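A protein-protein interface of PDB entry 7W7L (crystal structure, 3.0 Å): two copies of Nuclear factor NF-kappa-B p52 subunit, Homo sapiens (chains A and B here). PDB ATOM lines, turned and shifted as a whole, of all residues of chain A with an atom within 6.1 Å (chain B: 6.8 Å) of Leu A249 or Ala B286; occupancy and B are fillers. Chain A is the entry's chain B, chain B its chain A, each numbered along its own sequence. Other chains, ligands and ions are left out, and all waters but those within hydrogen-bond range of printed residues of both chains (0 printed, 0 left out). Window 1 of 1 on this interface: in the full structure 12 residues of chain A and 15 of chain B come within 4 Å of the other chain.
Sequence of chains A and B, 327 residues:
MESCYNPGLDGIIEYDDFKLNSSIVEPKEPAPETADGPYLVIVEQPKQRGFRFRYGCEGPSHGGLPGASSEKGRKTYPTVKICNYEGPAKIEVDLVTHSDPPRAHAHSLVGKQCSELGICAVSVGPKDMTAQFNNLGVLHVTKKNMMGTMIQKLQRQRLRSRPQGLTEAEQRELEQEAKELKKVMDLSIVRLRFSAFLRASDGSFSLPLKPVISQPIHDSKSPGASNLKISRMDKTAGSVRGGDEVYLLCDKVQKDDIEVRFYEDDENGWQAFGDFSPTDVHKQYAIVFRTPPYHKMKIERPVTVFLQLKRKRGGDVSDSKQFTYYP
A ring nitrogen (NE2) of His A282 lies within hydrogen-bond range of the backbone carbonyl oxygen (O) of Cys B250, at 2.9 Å. The backbone carbonyl oxygen of Tyr B285 is in hydrogen-bond range of a ring nitrogen (NE2) of His A282, 2.9 Å away. The backbone carbonyl oxygen of Tyr A285 sits close to a ring nitrogen (NE2) of His B282 (3.4 Å). A ring nitrogen (NE2) of His B282 lies within hydrogen-bond range of the backbone carbonyl oxygen (O) of Cys A250. The backbone carbonyl oxygen of Met A233 sits at hydrogen-bond distance from the side-chain hydroxyl of Tyr B247 (3.3 Å). The side-chain carboxylate (OD1) of Asp B280 lies within salt-bridge range of the guanidinium group (NH2) of Arg A232, 3.2 Å away.
The backbone NH (N) of Ser A231 lies within hydrogen-bond range of the backbone carbonyl oxygen (O) of Leu A249 (2.9 Å). The backbone NH of Val B288 sits at hydrogen-bond distance from the backbone carbonyl oxygen of Asp B280, 2.9 Å away. O of Tyr B285 lies within hydrogen-bond range of N of Cys B250 (3.0 Å). The backbone NH of Leu A249 lies within hydrogen-bond range of the backbone carbonyl oxygen of Arg A232, at 2.8 Å. O of Tyr A285 is in hydrogen-bond range of N of Cys A250, 3.0 Å away. SG of Cys A250 is in hydrogen-bond range of N of Ala A286 (3.5 Å).
Among the printed residues, pairs that only touch across the chains: Arg A232 with Val B288, Ser A231 with His B282, Tyr A285 with Tyr B285, Arg A232 with Tyr B247, Leu A249 with His B282, Tyr A247 with Tyr B247, His A282 with Leu B249, Leu A249 with Tyr B247, Leu A249 with Ala B286, Tyr A285 with Lys B283 and Tyr A247 with Leu B249.
Of the printed residues of chain B, Tyr A247 touches Tyr B247 and Leu B249. Printed residues of chain B within 4 Å of Leu A249: Tyr B247 (3.7 Å), His B282 (3.6 Å) and Ala B286 (3.8 Å). Of the printed residues of chain B, His A282 touches Leu B249 (3.7 Å), Cys B250 (2.9 Å) and Tyr B285 (2.9 Å). Printed residues of chain A within 4 Å of Leu B249: Tyr A247 (3.96 Å) and His A282 (3.7 Å). Of the printed residues of chain A, Cys B250 touches His A282. Val B281 touches none of the printed residues of chain A. Ala B286 touches one residue of chain A. The nearest printed residue of chain B that does not touch Leu A249 is Val B288 (4.01 Å). The nearest residue of chain A that does not touch Ala B286 is His A282 (5.1 Å).
Printed residues of chain B that touch a printed residue of chain A: Tyr B247, Leu B249, Cys B250, Asp B280, His B282, Lys B283, Tyr B285, Ala B286 and Val B288. Among the printed residues, Asp or Glu carboxylates within 4 Å of a Lys or Arg side-chain nitrogen of the other chain: Arg A232 with Asp B280.
Leu A249 touches Ala B286, but with the chains exchanged Ala A286 does not touch Leu B249 (4.03 Å). Cys A250 touches His B282, and with the chains exchanged His A282 touches Cys B250. His A282 touches Tyr B285, and with the chains exchanged Tyr A285 touches His B282. Tyr B285 touches its own counterpart, Tyr A285. Of the 17 pairs that touch across the chains among the printed residues, 10 have their exchanged pair printed and touching as well.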
ATOM      1  N   LYS A 229      36.334 -10.687   7.308  1.00  0.00           N
ATOM      2  CA  LYS A 229      35.437 -10.889   8.470  1.00  0.00           C
ATOM      3  C   LYS A 229      34.017 -10.506   8.073  1.00  0.00           C
ATOM      4  O   LYS A 229      33.858  -9.613   7.201  1.00  0.00           O
ATOM      5  CB  LYS A 229      35.936 -10.048   9.646  1.00  0.00           C
ATOM      6  CG  LYS A 229      35.251 -10.315  10.983  1.00  0.00           C
ATOM      7  CD  LYS A 229      35.192  -9.106  11.907  1.00  0.00           C
ATOM      8  CE  LYS A 229      33.960  -9.105  12.791  1.00  0.00           C
ATOM      9  NZ  LYS A 229      34.025  -8.063  13.839  1.00  0.00           N
ATOM     10  N   ILE A 230      33.047 -11.247   8.567  1.00  0.00           N
ATOM     11  CA  ILE A 230      31.625 -10.802   8.523  1.00  0.00           C
ATOM     12  C   ILE A 230      31.207 -10.308   9.908  1.00  0.00           C
ATOM     13  O   ILE A 230      31.475 -11.000  10.901  1.00  0.00           O
ATOM     14  CB  ILE A 230      30.651 -11.883   8.010  1.00  0.00           C
ATOM     15  CG1 ILE A 230      31.118 -12.498   6.688  1.00  0.00           C
ATOM     16  CG2 ILE A 230      29.256 -11.289   7.908  1.00  0.00           C
ATOM     17  CD1 ILE A 230      30.039 -13.083   5.806  1.00  0.00           C
ATOM     18  N   SER A 231      30.679  -9.105   9.951  1.00  0.00           N
ATOM     19  CA  SER A 231      30.213  -8.444  11.184  1.00  0.00           C
ATOM     20  C   SER A 231      28.819  -8.954  11.513  1.00  0.00           C
ATOM     21  O   SER A 231      28.653  -9.679  12.532  1.00  0.00           O
ATOM     22  CB  SER A 231      30.269  -6.951  11.037  1.00  0.00           C
ATOM     23  OG  SER A 231      31.599  -6.541  10.739  1.00  0.00           O
ATOM     24  N   ARG A 232      27.908  -8.675  10.599  1.00  0.00           N
ATOM     25  CA  ARG A 232      26.466  -8.863  10.773  1.00  0.00           C
ATOM     26  C   ARG A 232      25.751  -8.947   9.446  1.00  0.00           C
ATOM     27  O   ARG A 232      26.200  -8.355   8.467  1.00  0.00           O
ATOM     28  CB  ARG A 232      25.870  -7.645  11.482  1.00  0.00           C
ATOM     29  CG  ARG A 232      25.435  -7.904  12.910  1.00  0.00           C
ATOM     30  CD  ARG A 232      25.483  -6.606  13.679  1.00  0.00           C
ATOM     31  NE  ARG A 232      24.163  -6.081  13.948  1.00  0.00           N
ATOM     32  CZ  ARG A 232      23.937  -4.910  14.527  1.00  0.00           C
ATOM     33  NH1 ARG A 232      22.698  -4.531  14.776  1.00  0.00           N
ATOM     34  NH2 ARG A 232      24.942  -4.117  14.860  1.00  0.00           N
ATOM     35  N   MET A 233      24.566  -9.505   9.447  1.00  0.00           N
ATOM     36  CA  MET A 233      23.822  -9.705   8.197  1.00  0.00           C
ATOM     37  C   MET A 233      22.374  -9.487   8.530  1.00  0.00           C
ATOM     38  O   MET A 233      21.972  -9.908   9.624  1.00  0.00           O
ATOM     39  CB  MET A 233      24.007 -11.167   7.811  1.00  0.00           C
ATOM     40  CG  MET A 233      23.634 -11.514   6.414  1.00  0.00           C
ATOM     41  SD  MET A 233      24.237 -13.184   6.044  1.00  0.00           S
ATOM     42  CE  MET A 233      25.725 -13.247   7.051  1.00  0.00           C
ATOM     43  N   TYR A 247      21.677  -7.755   3.270  1.00  0.00           N
ATOM     44  CA  TYR A 247      22.659  -6.700   3.593  1.00  0.00           C
ATOM     45  C   TYR A 247      23.694  -7.365   4.474  1.00  0.00           C
ATOM     46  O   TYR A 247      23.370  -7.770   5.572  1.00  0.00           O
ATOM     47  CB  TYR A 247      21.998  -5.548   4.353  1.00  0.00           C
ATOM     48  CG  TYR A 247      21.261  -4.541   3.508  1.00  0.00           C
ATOM     49  CD1 TYR A 247      20.526  -4.910   2.393  1.00  0.00           C
ATOM     50  CD2 TYR A 247      21.265  -3.206   3.859  1.00  0.00           C
ATOM     51  CE1 TYR A 247      19.849  -3.976   1.630  1.00  0.00           C
ATOM     52  CE2 TYR A 247      20.583  -2.254   3.114  1.00  0.00           C
ATOM     53  CZ  TYR A 247      19.870  -2.642   1.996  1.00  0.00           C
ATOM     54  OH  TYR A 247      19.191  -1.713   1.264  1.00  0.00           O
ATOM     55  N   LEU A 248      24.927  -7.438   4.003  1.00  0.00           N
ATOM     56  CA  LEU A 248      26.043  -8.042   4.763  1.00  0.00           C
ATOM     57  C   LEU A 248      26.980  -6.915   5.180  1.00  0.00           C
ATOM     58  O   LEU A 248      27.430  -6.190   4.314  1.00  0.00           O
ATOM     59  CB  LEU A 248      26.754  -9.012   3.817  1.00  0.00           C
ATOM     60  CG  LEU A 248      27.932  -9.769   4.411  1.00  0.00           C
ATOM     61  CD1 LEU A 248      27.451 -10.592   5.590  1.00  0.00           C
ATOM     62  CD2 LEU A 248      28.579 -10.635   3.350  1.00  0.00           C
ATOM     63  N   LEU A 249      27.295  -6.784   6.456  1.00  0.00           N
ATOM     64  CA  LEU A 249      28.308  -5.811   6.901  1.00  0.00           C
ATOM     65  C   LEU A 249      29.602  -6.568   7.073  1.00  0.00           C
ATOM     66  O   LEU A 249      29.634  -7.585   7.762  1.00  0.00           O
ATOM     67  CB  LEU A 249      27.822  -5.112   8.169  1.00  0.00           C
ATOM     68  CG  LEU A 249      26.505  -4.349   7.995  1.00  0.00           C
ATOM     69  CD1 LEU A 249      26.168  -3.552   9.243  1.00  0.00           C
ATOM     70  CD2 LEU A 249      26.540  -3.431   6.780  1.00  0.00           C
ATOM     71  N   CYS A 250      30.674  -6.100   6.462  1.00  0.00           N
ATOM     72  CA  CYS A 250      31.945  -6.867   6.382  1.00  0.00           C
ATOM     73  C   CYS A 250      33.163  -5.985   6.720  1.00  0.00           C
ATOM     74  O   CYS A 250      33.022  -4.768   6.854  1.00  0.00           O
ATOM     75  CB  CYS A 250      32.122  -7.392   4.964  1.00  0.00           C
ATOM     76  SG  CYS A 250      31.932  -6.095   3.705  1.00  0.00           S
ATOM     77  N   ASP A 251      34.332  -6.605   6.882  1.00  0.00           N
ATOM     78  CA  ASP A 251      35.576  -5.827   6.973  1.00  0.00           C
ATOM     79  C   ASP A 251      35.748  -5.240   5.582  1.00  0.00           C
ATOM     80  O   ASP A 251      34.810  -5.335   4.753  1.00  0.00           O
ATOM     81  CB  ASP A 251      36.715  -6.667   7.545  1.00  0.00           C
ATOM     82  CG  ASP A 251      36.658  -6.706   9.066  1.00  0.00           C
ATOM     83  OD1 ASP A 251      35.621  -6.272   9.635  1.00  0.00           O
ATOM     84  OD2 ASP A 251      37.649  -7.155   9.682  1.00  0.00           O
ATOM     85  N   HIS A 282      29.183  -1.577  -0.966  1.00  0.00           N
ATOM     86  CA  HIS A 282      29.113  -0.180  -0.451  1.00  0.00           C
ATOM     87  C   HIS A 282      30.350   0.263   0.342  1.00  0.00           C
ATOM     88  O   HIS A 282      30.568  -0.240   1.481  1.00  0.00           O
ATOM     89  CB  HIS A 282      27.872  -0.026   0.441  1.00  0.00           C
ATOM     90  CG  HIS A 282      27.781   1.206   1.279  1.00  0.00           C
ATOM     91  ND1 HIS A 282      26.997   2.293   0.909  1.00  0.00           N
ATOM     92  CD2 HIS A 282      28.257   1.493   2.511  1.00  0.00           C
ATOM     93  CE1 HIS A 282      27.047   3.219   1.845  1.00  0.00           C
ATOM     94  NE2 HIS A 282      27.819   2.755   2.840  1.00  0.00           N
ATOM     95  N   TYR A 285      32.688  -1.859   2.817  1.00  0.00           N
ATOM     96  CA  TYR A 285      32.301  -2.355   4.164  1.00  0.00           C
ATOM     97  C   TYR A 285      30.893  -2.960   4.264  1.00  0.00           C
ATOM     98  O   TYR A 285      30.404  -3.288   5.363  1.00  0.00           O
ATOM     99  CB  TYR A 285      32.487  -1.227   5.190  1.00  0.00           C
ATOM    100  CG  TYR A 285      33.922  -0.823   5.455  1.00  0.00           C
ATOM    101  CD1 TYR A 285      34.855  -1.730   5.937  1.00  0.00           C
ATOM    102  CD2 TYR A 285      34.350   0.479   5.252  1.00  0.00           C
ATOM    103  CE1 TYR A 285      36.167  -1.358   6.186  1.00  0.00           C
ATOM    104  CE2 TYR A 285      35.660   0.866   5.493  1.00  0.00           C
ATOM    105  CZ  TYR A 285      36.578  -0.059   5.954  1.00  0.00           C
ATOM    106  OH  TYR A 285      37.873   0.311   6.184  1.00  0.00           O
ATOM    107  N   ALA A 286      30.200  -3.066   3.145  1.00  0.00           N
ATOM    108  CA  ALA A 286      28.858  -3.649   3.103  1.00  0.00           C
ATOM    109  C   ALA A 286      28.652  -4.186   1.709  1.00  0.00           C
ATOM    110  O   ALA A 286      29.227  -3.677   0.752  1.00  0.00           O
ATOM    111  CB  ALA A 286      27.817  -2.630   3.497  1.00  0.00           C
ATOM    112  N   ILE A 287      27.862  -5.238   1.633  1.00  0.00           N
ATOM    113  CA  ILE A 287      27.511  -5.924   0.375  1.00  0.00           C
ATOM    114  C   ILE A 287      26.001  -6.138   0.372  1.00  0.00           C
ATOM    115  O   ILE A 287      25.463  -6.704   1.310  1.00  0.00           O
ATOM    116  CB  ILE A 287      28.291  -7.235   0.157  1.00  0.00           C
ATOM    117  CG1 ILE A 287      29.733  -7.162   0.667  1.00  0.00           C
ATOM    118  CG2 ILE A 287      28.237  -7.584  -1.319  1.00  0.00           C
ATOM    119  CD1 ILE A 287      30.501  -8.451   0.508  1.00  0.00           C
ATOM    120  N   TYR B 247      18.700  -1.648   8.608  1.00  0.00           N
ATOM    121  CA  TYR B 247      20.104  -1.461   8.184  1.00  0.00           C
ATOM    122  C   TYR B 247      20.095  -0.274   7.244  1.00  0.00           C
ATOM    123  O   TYR B 247      19.508  -0.363   6.177  1.00  0.00           O
ATOM    124  CB  TYR B 247      20.653  -2.672   7.428  1.00  0.00           C
ATOM    125  CG  TYR B 247      21.162  -3.785   8.297  1.00  0.00           C
ATOM    126  CD1 TYR B 247      20.388  -4.315   9.314  1.00  0.00           C
ATOM    127  CD2 TYR B 247      22.425  -4.317   8.092  1.00  0.00           C
ATOM    128  CE1 TYR B 247      20.851  -5.364  10.093  1.00  0.00           C
ATOM    129  CE2 TYR B 247      22.911  -5.348   8.879  1.00  0.00           C
ATOM    130  CZ  TYR B 247      22.125  -5.873   9.889  1.00  0.00           C
ATOM    131  OH  TYR B 247      22.633  -6.880  10.661  1.00  0.00           O
ATOM    132  N   LEU B 248      20.777   0.791   7.615  1.00  0.00           N
ATOM    133  CA  LEU B 248      20.872   2.015   6.793  1.00  0.00           C
ATOM    134  C   LEU B 248      22.293   2.120   6.267  1.00  0.00           C
ATOM    135  O   LEU B 248      23.203   2.108   7.080  1.00  0.00           O
ATOM    136  CB  LEU B 248      20.513   3.217   7.662  1.00  0.00           C
ATOM    137  CG  LEU B 248      20.295   4.517   6.891  1.00  0.00           C
ATOM    138  CD1 LEU B 248      19.153   5.327   7.498  1.00  0.00           C
ATOM    139  CD2 LEU B 248      21.566   5.347   6.833  1.00  0.00           C
ATOM    140  N   LEU B 249      22.492   2.232   4.961  1.00  0.00           N
ATOM    141  CA  LEU B 249      23.856   2.429   4.420  1.00  0.00           C
ATOM    142  C   LEU B 249      24.001   3.910   4.141  1.00  0.00           C
ATOM    143  O   LEU B 249      23.139   4.528   3.508  1.00  0.00           O
ATOM    144  CB  LEU B 249      24.015   1.557   3.173  1.00  0.00           C
ATOM    145  CG  LEU B 249      23.800   0.061   3.419  1.00  0.00           C
ATOM    146  CD1 LEU B 249      24.128  -0.749   2.175  1.00  0.00           C
ATOM    147  CD2 LEU B 249      24.629  -0.427   4.606  1.00  0.00           C
ATOM    148  N   CYS B 250      25.067   4.513   4.651  1.00  0.00           N
ATOM    149  CA  CYS B 250      25.293   5.970   4.462  1.00  0.00           C
ATOM    150  C   CYS B 250      26.717   6.315   4.017  1.00  0.00           C
ATOM    151  O   CYS B 250      27.548   5.446   3.911  1.00  0.00           O
ATOM    152  CB  CYS B 250      24.937   6.733   5.731  1.00  0.00           C
ATOM    153  SG  CYS B 250      25.850   6.190   7.195  1.00  0.00           S
ATOM    154  N   ASP B 251      26.972   7.586   3.723  1.00  0.00           N
ATOM    155  CA  ASP B 251      28.347   8.068   3.498  1.00  0.00           C
ATOM    156  C   ASP B 251      28.967   8.148   4.872  1.00  0.00           C
ATOM    157  O   ASP B 251      28.247   8.149   5.899  1.00  0.00           O
ATOM    158  CB  ASP B 251      28.403   9.390   2.731  1.00  0.00           C
ATOM    159  CG  ASP B 251      28.059   9.231   1.261  1.00  0.00           C
ATOM    160  OD1 ASP B 251      27.966   8.081   0.811  1.00  0.00           O
ATOM    161  OD2 ASP B 251      27.835  10.253   0.596  1.00  0.00           O
ATOM    162  N   VAL B 253      30.153   8.661   8.459  1.00  0.00           N
ATOM    163  CA  VAL B 253      29.659   9.486   9.580  1.00  0.00           C
ATOM    164  C   VAL B 253      30.486   9.181  10.821  1.00  0.00           C
ATOM    165  O   VAL B 253      31.116   8.105  10.941  1.00  0.00           O
ATOM    166  CB  VAL B 253      28.161   9.274   9.866  1.00  0.00           C
ATOM    167  CG1 VAL B 253      27.305   9.652   8.665  1.00  0.00           C
ATOM    168  CG2 VAL B 253      27.862   7.860  10.345  1.00  0.00           C
ATOM    169  N   ASP B 280      26.595  -0.195  16.812  1.00  0.00           N
ATOM    170  CA  ASP B 280      25.585  -0.346  15.763  1.00  0.00           C
ATOM    171  C   ASP B 280      25.929   0.477  14.524  1.00  0.00           C
ATOM    172  O   ASP B 280      25.307   0.265  13.483  1.00  0.00           O
ATOM    173  CB  ASP B 280      24.171  -0.072  16.289  1.00  0.00           C
ATOM    174  CG  ASP B 280      23.597  -1.206  17.123  1.00  0.00           C
ATOM    175  OD1 ASP B 280      24.317  -2.209  17.315  1.00  0.00           O
ATOM    176  OD2 ASP B 280      22.430  -1.078  17.575  1.00  0.00           O
ATOM    177  N   VAL B 281      26.809   1.452  14.682  1.00  0.00           N
ATOM    178  CA  VAL B 281      27.310   2.222  13.542  1.00  0.00           C
ATOM    179  C   VAL B 281      28.522   1.451  13.086  1.00  0.00           C
ATOM    180  O   VAL B 281      29.548   1.535  13.736  1.00  0.00           O
ATOM    181  CB  VAL B 281      27.632   3.685  13.897  1.00  0.00           C
ATOM    182  CG1 VAL B 281      28.470   4.343  12.810  1.00  0.00           C
ATOM    183  CG2 VAL B 281      26.366   4.487  14.176  1.00  0.00           C
ATOM    184  N   HIS B 282      28.377   0.782  11.943  1.00  0.00           N
ATOM    185  CA  HIS B 282      29.418  -0.100  11.357  1.00  0.00           C
ATOM    186  C   HIS B 282      30.441   0.617  10.467  1.00  0.00           C
ATOM    187  O   HIS B 282      30.070   1.053   9.350  1.00  0.00           O
ATOM    188  CB  HIS B 282      28.787  -1.222  10.523  1.00  0.00           C
ATOM    189  CG  HIS B 282      29.824  -2.134   9.945  1.00  0.00           C
ATOM    190  ND1 HIS B 282      30.748  -2.799  10.741  1.00  0.00           N
ATOM    191  CD2 HIS B 282      30.143  -2.437   8.670  1.00  0.00           C
ATOM    192  CE1 HIS B 282      31.564  -3.504   9.978  1.00  0.00           C
ATOM    193  NE2 HIS B 282      31.202  -3.310   8.699  1.00  0.00           N
ATOM    194  N   LYS B 283      31.704   0.675  10.906  1.00  0.00           N
ATOM    195  CA  LYS B 283      32.840   1.215  10.113  1.00  0.00           C
ATOM    196  C   LYS B 283      32.451   2.517   9.395  1.00  0.00           C
ATOM    197  O   LYS B 283      32.797   2.705   8.222  1.00  0.00           O
ATOM    198  CB  LYS B 283      33.335   0.149   9.134  1.00  0.00           C
ATOM    199  CG  LYS B 283      33.905  -1.093   9.790  1.00  0.00           C
ATOM    200  CD  LYS B 283      34.600  -0.829  11.108  1.00  0.00           C
ATOM    201  CE  LYS B 283      35.373  -2.026  11.615  1.00  0.00           C
ATOM    202  NZ  LYS B 283      36.430  -2.441  10.660  1.00  0.00           N
ATOM    203  N   GLN B 284      31.720   3.378  10.096  1.00  0.00           N
ATOM    204  CA  GLN B 284      31.289   4.728   9.660  1.00  0.00           C
ATOM    205  C   GLN B 284      30.455   4.788   8.381  1.00  0.00           C
ATOM    206  O   GLN B 284      30.157   5.892   7.897  1.00  0.00           O
ATOM    207  CB  GLN B 284      32.541   5.582   9.471  1.00  0.00           C
ATOM    208  CG  GLN B 284      33.356   5.746  10.750  1.00  0.00           C
ATOM    209  CD  GLN B 284      34.743   6.309  10.545  1.00  0.00           C
ATOM    210  OE1 GLN B 284      35.515   5.867   9.687  1.00  0.00           O
ATOM    211  NE2 GLN B 284      35.081   7.292  11.363  1.00  0.00           N
ATOM    212  N   TYR B 285      30.008   3.648   7.878  1.00  0.00           N
ATOM    213  CA  TYR B 285      29.223   3.585   6.616  1.00  0.00           C
ATOM    214  C   TYR B 285      27.855   2.879   6.710  1.00  0.00           C
ATOM    215  O   TYR B 285      27.216   2.627   5.677  1.00  0.00           O
ATOM    216  CB  TYR B 285      30.095   2.917   5.552  1.00  0.00           C
ATOM    217  CG  TYR B 285      31.270   3.736   5.077  1.00  0.00           C
ATOM    218  CD1 TYR B 285      31.092   4.986   4.508  1.00  0.00           C
ATOM    219  CD2 TYR B 285      32.563   3.244   5.153  1.00  0.00           C
ATOM    220  CE1 TYR B 285      32.165   5.728   4.040  1.00  0.00           C
ATOM    221  CE2 TYR B 285      33.649   3.966   4.685  1.00  0.00           C
ATOM    222  CZ  TYR B 285      33.449   5.213   4.114  1.00  0.00           C
ATOM    223  OH  TYR B 285      34.492   5.963   3.639  1.00  0.00           O
ATOM    224  N   ALA B 286      27.455   2.475   7.904  1.00  0.00           N
ATOM    225  CA  ALA B 286      26.190   1.749   8.064  1.00  0.00           C
ATOM    226  C   ALA B 286      25.747   1.930   9.491  1.00  0.00           C
ATOM    227  O   ALA B 286      26.585   2.063  10.364  1.00  0.00           O
ATOM    228  CB  ALA B 286      26.328   0.288   7.695  1.00  0.00           C
ATOM    229  N   ILE B 287      24.441   1.952   9.672  1.00  0.00           N
ATOM    230  CA  ILE B 287      23.793   2.114  10.990  1.00  0.00           C
ATOM    231  C   ILE B 287      22.711   1.041  11.107  1.00  0.00           C
ATOM    232  O   ILE B 287      21.854   0.946  10.239  1.00  0.00           O
ATOM    233  CB  ILE B 287      23.204   3.535  11.127  1.00  0.00           C
ATOM    234  CG1 ILE B 287      24.238   4.607  10.778  1.00  0.00           C
ATOM    235  CG2 ILE B 287      22.596   3.778  12.507  1.00  0.00           C
ATOM    236  CD1 ILE B 287      23.669   6.004  10.710  1.00  0.00           C
ATOM    237  N   VAL B 288      22.779   0.238  12.152  1.00  0.00           N
ATOM    238  CA  VAL B 288      21.719  -0.753  12.431  1.00  0.00           C
ATOM    239  C   VAL B 288      20.949  -0.140  13.564  1.00  0.00           C
ATOM    240  O   VAL B 288      21.487  -0.020  14.648  1.00  0.00           O
ATOM    241  CB  VAL B 288      22.233  -2.162  12.771  1.00  0.00           C
ATOM    242  CG1 VAL B 288      21.057  -3.061  13.122  1.00  0.00           C
ATOM    243  CG2 VAL B 288      23.053  -2.754  11.635  1.00  0.00           C
